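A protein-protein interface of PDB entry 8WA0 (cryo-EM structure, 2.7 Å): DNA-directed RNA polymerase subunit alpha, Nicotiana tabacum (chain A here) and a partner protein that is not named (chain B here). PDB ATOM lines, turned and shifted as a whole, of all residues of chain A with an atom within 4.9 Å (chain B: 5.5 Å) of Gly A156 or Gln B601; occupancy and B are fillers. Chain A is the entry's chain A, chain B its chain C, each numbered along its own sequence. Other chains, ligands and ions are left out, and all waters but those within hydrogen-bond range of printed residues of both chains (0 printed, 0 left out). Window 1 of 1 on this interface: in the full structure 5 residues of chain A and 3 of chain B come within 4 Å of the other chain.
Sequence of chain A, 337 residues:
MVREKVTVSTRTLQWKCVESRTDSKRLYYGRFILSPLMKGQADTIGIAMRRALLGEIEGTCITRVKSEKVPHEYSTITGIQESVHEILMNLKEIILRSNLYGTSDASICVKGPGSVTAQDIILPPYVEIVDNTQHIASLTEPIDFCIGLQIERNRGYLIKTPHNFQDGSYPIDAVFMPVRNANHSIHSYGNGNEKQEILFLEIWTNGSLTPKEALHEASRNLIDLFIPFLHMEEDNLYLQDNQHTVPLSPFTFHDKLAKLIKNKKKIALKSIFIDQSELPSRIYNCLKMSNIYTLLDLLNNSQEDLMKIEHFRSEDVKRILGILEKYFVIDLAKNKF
The backbone NH (N) of Leu A158 lies close to the guanidinium group (NH2) of Arg B603 (3.4 Å).
The backbone carbonyl oxygen (O) of Gly A156 lies within hydrogen-bond range of the side-chain amide nitrogen (NE2) of Gln B601 (3.0 Å).
The backbone carbonyl oxygen of Gly A156 is in hydrogen-bond range of the guanidinium group of Arg B603, at 3.0 Å.
OE1 of Gln B601 sits at hydrogen-bond distance from NE of Arg B603 (3.2 Å).
The backbone NH (N) of Arg B603 lies within hydrogen-bond range of the backbone carbonyl oxygen (O) of Ala B598, at 2.9 Å.
Among the printed residues, merely in contact across the chains: Leu A54 with Arg B600 (3.5 Å), Leu A158 with Gln B601 (3.5 Å) and Tyr A157 with Arg B603 (3.8 Å).
Printed residues of chain B within 4 Å of Leu A54: Arg B600 (3.5 Å).
Gly A156 touches two residues of chain B.
Of the printed residues of chain B, Tyr A157 touches Arg B603 (3.8 Å).
Of the printed residues of chain B, Leu A158 touches Gln B601 and Arg B603.
Phe A176 touches none of the printed residues of chain B.
Gly B597 touches none of the printed residues of chain A.
Printed residues of chain A within 4 Å of Arg B600: Leu A54.
Gln B601 touches two residues of chain A.
Printed residues of chain A within 4 Å of Arg B603: Gly A156 (3.0 Å), Tyr A157 (3.8 Å) and Leu A158 (3.4 Å).
The nearest printed residue of chain B that does not touch Gly A156 is Lys B602 (9.3 Å).
The nearest residue of chain A that does not touch Gln B601 is Leu A54 (4.5 Å).
Of the 9 printed residues of chain A, 4 touch a printed residue of chain B.
Hydrophobic or aromatic side chains of chain A within 4 Å of the printed part of chain B: Leu A54 and Leu A158.
Among the printed residues, no Asp or Glu carboxylate lies within 4 Å of a Lys or Arg side-chain nitrogen of the other chain.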
ATOM      1  N   LEU A  54     -19.184   5.190  11.715  1.00  0.00           N
ATOM      2  CA  LEU A  54     -20.341   6.014  11.991  1.00  0.00           C
ATOM      3  C   LEU A  54     -20.342   7.342  11.258  1.00  0.00           C
ATOM      4  O   LEU A  54     -21.390   7.942  11.109  1.00  0.00           O
ATOM      5  CB  LEU A  54     -20.518   6.200  13.485  1.00  0.00           C
ATOM      6  CG  LEU A  54     -20.968   4.940  14.216  1.00  0.00           C
ATOM      7  CD1 LEU A  54     -20.726   5.056  15.708  1.00  0.00           C
ATOM      8  CD2 LEU A  54     -22.426   4.649  13.916  1.00  0.00           C
ATOM      9  N   ILE A  57     -18.457   6.629   6.038  1.00  0.00           N
ATOM     10  CA  ILE A  57     -19.092   5.853   4.984  1.00  0.00           C
ATOM     11  C   ILE A  57     -20.160   6.693   4.314  1.00  0.00           C
ATOM     12  O   ILE A  57     -20.812   7.477   4.977  1.00  0.00           O
ATOM     13  CB  ILE A  57     -19.658   4.545   5.554  1.00  0.00           C
ATOM     14  CG1 ILE A  57     -18.545   3.755   6.228  1.00  0.00           C
ATOM     15  CG2 ILE A  57     -20.298   3.697   4.472  1.00  0.00           C
ATOM     16  CD1 ILE A  57     -18.979   2.386   6.679  1.00  0.00           C
ATOM     17  N   ASN A 154     -24.135  11.467   0.115  1.00  0.00           N
ATOM     18  CA  ASN A 154     -23.201  12.184   0.989  1.00  0.00           C
ATOM     19  C   ASN A 154     -22.839  11.334   2.208  1.00  0.00           C
ATOM     20  O   ASN A 154     -23.575  10.417   2.562  1.00  0.00           O
ATOM     21  CB  ASN A 154     -23.806  13.518   1.429  1.00  0.00           C
ATOM     22  CG  ASN A 154     -22.756  14.535   1.834  1.00  0.00           C
ATOM     23  OD1 ASN A 154     -21.556  14.298   1.697  1.00  0.00           O
ATOM     24  ND2 ASN A 154     -23.207  15.681   2.328  1.00  0.00           N
ATOM     25  N   ARG A 155     -21.708  11.627   2.846  1.00  0.00           N
ATOM     26  CA  ARG A 155     -21.271  10.848   4.008  1.00  0.00           C
ATOM     27  C   ARG A 155     -21.880  11.283   5.336  1.00  0.00           C
ATOM     28  O   ARG A 155     -21.193  11.865   6.176  1.00  0.00           O
ATOM     29  CB  ARG A 155     -19.742  10.842   4.118  1.00  0.00           C
ATOM     30  CG  ARG A 155     -19.066  12.150   3.742  1.00  0.00           C
ATOM     31  CD  ARG A 155     -17.576  12.089   4.038  1.00  0.00           C
ATOM     32  NE  ARG A 155     -17.309  11.898   5.461  1.00  0.00           N
ATOM     33  CZ  ARG A 155     -17.025  12.883   6.309  1.00  0.00           C
ATOM     34  NH1 ARG A 155     -16.957  14.135   5.878  1.00  0.00           N
ATOM     35  NH2 ARG A 155     -16.801  12.615   7.587  1.00  0.00           N
ATOM     36  N   GLY A 156     -23.160  10.996   5.540  1.00  0.00           N
ATOM     37  CA  GLY A 156     -23.796  11.310   6.809  1.00  0.00           C
ATOM     38  C   GLY A 156     -23.766  12.755   7.263  1.00  0.00           C
ATOM     39  O   GLY A 156     -23.612  13.019   8.455  1.00  0.00           O
ATOM     40  N   TYR A 157     -23.542  13.652   6.309  1.00  0.00           N
ATOM     41  CA  TYR A 157     -23.501  15.073   6.635  1.00  0.00           C
ATOM     42  C   TYR A 157     -24.944  15.391   6.526  1.00  0.00           C
ATOM     43  O   TYR A 157     -25.492  15.442   5.431  1.00  0.00           O
ATOM     44  CB  TYR A 157     -22.675  15.877   5.645  1.00  0.00           C
ATOM     45  N   LEU A 158     -25.577  15.645   7.649  1.00  0.00           N
ATOM     46  CA  LEU A 158     -27.009  15.786   7.621  1.00  0.00           C
ATOM     47  C   LEU A 158     -27.602  16.883   6.760  1.00  0.00           C
ATOM     48  O   LEU A 158     -28.597  16.647   6.077  1.00  0.00           O
ATOM     49  CB  LEU A 158     -27.529  15.895   9.055  1.00  0.00           C
ATOM     50  CG  LEU A 158     -28.020  14.596   9.695  1.00  0.00           C
ATOM     51  CD1 LEU A 158     -26.929  13.540   9.776  1.00  0.00           C
ATOM     52  CD2 LEU A 158     -28.636  14.852  11.060  1.00  0.00           C
ATOM     53  N   PHE A 176     -27.717  10.620   6.400  1.00  0.00           N
ATOM     54  CA  PHE A 176     -27.135   9.837   5.334  1.00  0.00           C
ATOM     55  C   PHE A 176     -26.350   8.671   5.869  1.00  0.00           C
ATOM     56  O   PHE A 176     -25.500   8.155   5.167  1.00  0.00           O
ATOM     57  CB  PHE A 176     -26.183  10.672   4.507  1.00  0.00           C
ATOM     58  CG  PHE A 176     -26.821  11.646   3.574  1.00  0.00           C
ATOM     59  CD1 PHE A 176     -27.144  12.913   3.996  1.00  0.00           C
ATOM     60  CD2 PHE A 176     -27.001  11.323   2.250  1.00  0.00           C
ATOM     61  CE1 PHE A 176     -27.689  13.829   3.122  1.00  0.00           C
ATOM     62  CE2 PHE A 176     -27.541  12.230   1.366  1.00  0.00           C
ATOM     63  CZ  PHE A 176     -27.890  13.487   1.803  1.00  0.00           C
ATOM     64  N   MET A 177     -26.589   8.261   7.104  1.00  0.00           N
ATOM     65  CA  MET A 177     -25.775   7.212   7.715  1.00  0.00           C
ATOM     66  C   MET A 177     -26.209   5.777   7.489  1.00  0.00           C
ATOM     67  O   MET A 177     -27.223   5.353   8.018  1.00  0.00           O
ATOM     68  CB  MET A 177     -25.794   7.455   9.212  1.00  0.00           C
ATOM     69  CG  MET A 177     -24.610   6.916   9.984  1.00  0.00           C
ATOM     70  SD  MET A 177     -24.729   7.450  11.700  1.00  0.00           S
ATOM     71  CE  MET A 177     -26.386   6.905  12.105  1.00  0.00           C
ATOM     72  N   GLY B 597     -28.854   8.517  18.680  1.00  0.00           N
ATOM     73  CA  GLY B 597     -27.834   8.666  17.685  1.00  0.00           C
ATOM     74  C   GLY B 597     -27.399  10.067  17.406  1.00  0.00           C
ATOM     75  O   GLY B 597     -26.224  10.303  17.185  1.00  0.00           O
ATOM     76  N   ALA B 598     -28.324  11.004  17.408  1.00  0.00           N
ATOM     77  CA  ALA B 598     -27.971  12.358  17.079  1.00  0.00           C
ATOM     78  C   ALA B 598     -27.102  12.912  18.164  1.00  0.00           C
ATOM     79  O   ALA B 598     -26.253  13.748  17.912  1.00  0.00           O
ATOM     80  CB  ALA B 598     -29.205  13.192  16.934  1.00  0.00           C
ATOM     81  N   TYR B 599     -27.310  12.447  19.382  1.00  0.00           N
ATOM     82  CA  TYR B 599     -26.531  12.939  20.494  1.00  0.00           C
ATOM     83  C   TYR B 599     -25.096  12.574  20.270  1.00  0.00           C
ATOM     84  O   TYR B 599     -24.201  13.359  20.545  1.00  0.00           O
ATOM     85  CB  TYR B 599     -27.020  12.347  21.803  1.00  0.00           C
ATOM     86  CG  TYR B 599     -26.322  12.872  23.025  1.00  0.00           C
ATOM     87  CD1 TYR B 599     -26.189  14.232  23.238  1.00  0.00           C
ATOM     88  CD2 TYR B 599     -25.814  12.007  23.975  1.00  0.00           C
ATOM     89  CE1 TYR B 599     -25.551  14.715  24.358  1.00  0.00           C
ATOM     90  CE2 TYR B 599     -25.179  12.482  25.103  1.00  0.00           C
ATOM     91  CZ  TYR B 599     -25.050  13.837  25.289  1.00  0.00           C
ATOM     92  OH  TYR B 599     -24.415  14.314  26.412  1.00  0.00           O
ATOM     93  N   ARG B 600     -24.862  11.376  19.768  1.00  0.00           N
ATOM     94  CA  ARG B 600     -23.508  10.928  19.553  1.00  0.00           C
ATOM     95  C   ARG B 600     -22.854  11.696  18.426  1.00  0.00           C
ATOM     96  O   ARG B 600     -21.707  12.109  18.536  1.00  0.00           O
ATOM     97  CB  ARG B 600     -23.506   9.443  19.243  1.00  0.00           C
ATOM     98  CG  ARG B 600     -24.192   8.604  20.306  1.00  0.00           C
ATOM     99  CD  ARG B 600     -24.061   7.112  20.040  1.00  0.00           C
ATOM    100  NE  ARG B 600     -24.967   6.622  19.003  1.00  0.00           N
ATOM    101  CZ  ARG B 600     -24.622   6.413  17.736  1.00  0.00           C
ATOM    102  NH1 ARG B 600     -23.384   6.652  17.336  1.00  0.00           N
ATOM    103  NH2 ARG B 600     -25.516   5.961  16.868  1.00  0.00           N
ATOM    104  N   GLN B 601     -23.577  11.902  17.342  1.00  0.00           N
ATOM    105  CA  GLN B 601     -23.021  12.588  16.199  1.00  0.00           C
ATOM    106  C   GLN B 601     -22.945  14.060  16.454  1.00  0.00           C
ATOM    107  O   GLN B 601     -22.540  14.804  15.573  1.00  0.00           O
ATOM    108  CB  GLN B 601     -23.904  12.329  14.995  1.00  0.00           C
ATOM    109  CG  GLN B 601     -23.165  12.223  13.672  1.00  0.00           C
ATOM    110  CD  GLN B 601     -24.106  12.156  12.485  1.00  0.00           C
ATOM    111  OE1 GLN B 601     -25.320  12.302  12.633  1.00  0.00           O
ATOM    112  NE2 GLN B 601     -23.550  11.941  11.299  1.00  0.00           N
ATOM    113  N   LYS B 602     -23.269  14.472  17.684  1.00  0.00           N
ATOM    114  CA  LYS B 602     -23.208  15.886  18.091  1.00  0.00           C
ATOM    115  C   LYS B 602     -24.208  16.793  17.395  1.00  0.00           C
ATOM    116  O   LYS B 602     -24.070  18.014  17.434  1.00  0.00           O
ATOM    117  CB  LYS B 602     -21.781  16.453  18.016  1.00  0.00           C
ATOM    118  CG  LYS B 602     -20.814  15.807  18.994  1.00  0.00           C
ATOM    119  CD  LYS B 602     -19.452  16.480  18.948  1.00  0.00           C
ATOM    120  CE  LYS B 602     -18.503  15.871  19.967  1.00  0.00           C
ATOM    121  NZ  LYS B 602     -17.192  16.577  19.994  1.00  0.00           N
ATOM    122  N   ARG B 603     -25.214  16.206  16.762  1.00  0.00           N
ATOM    123  CA  ARG B 603     -26.257  17.012  16.141  1.00  0.00           C
ATOM    124  C   ARG B 603     -27.023  17.804  17.196  1.00  0.00           C
ATOM    125  O   ARG B 603     -27.339  18.974  16.987  1.00  0.00           O
ATOM    126  CB  ARG B 603     -27.206  16.129  15.333  1.00  0.00           C
ATOM    127  CG  ARG B 603     -26.507  15.327  14.249  1.00  0.00           C
ATOM    128  CD  ARG B 603     -25.815  16.241  13.250  1.00  0.00           C
ATOM    129  NE  ARG B 603     -25.033  15.493  12.272  1.00  0.00           N
ATOM    130  CZ  ARG B 603     -24.386  16.046  11.252  1.00  0.00           C
ATOM    131  NH1 ARG B 603     -24.429  17.359  11.070  1.00  0.00           N
ATOM    132  NH2 ARG B 603     -23.699  15.288  10.411  1.00  0.00           N
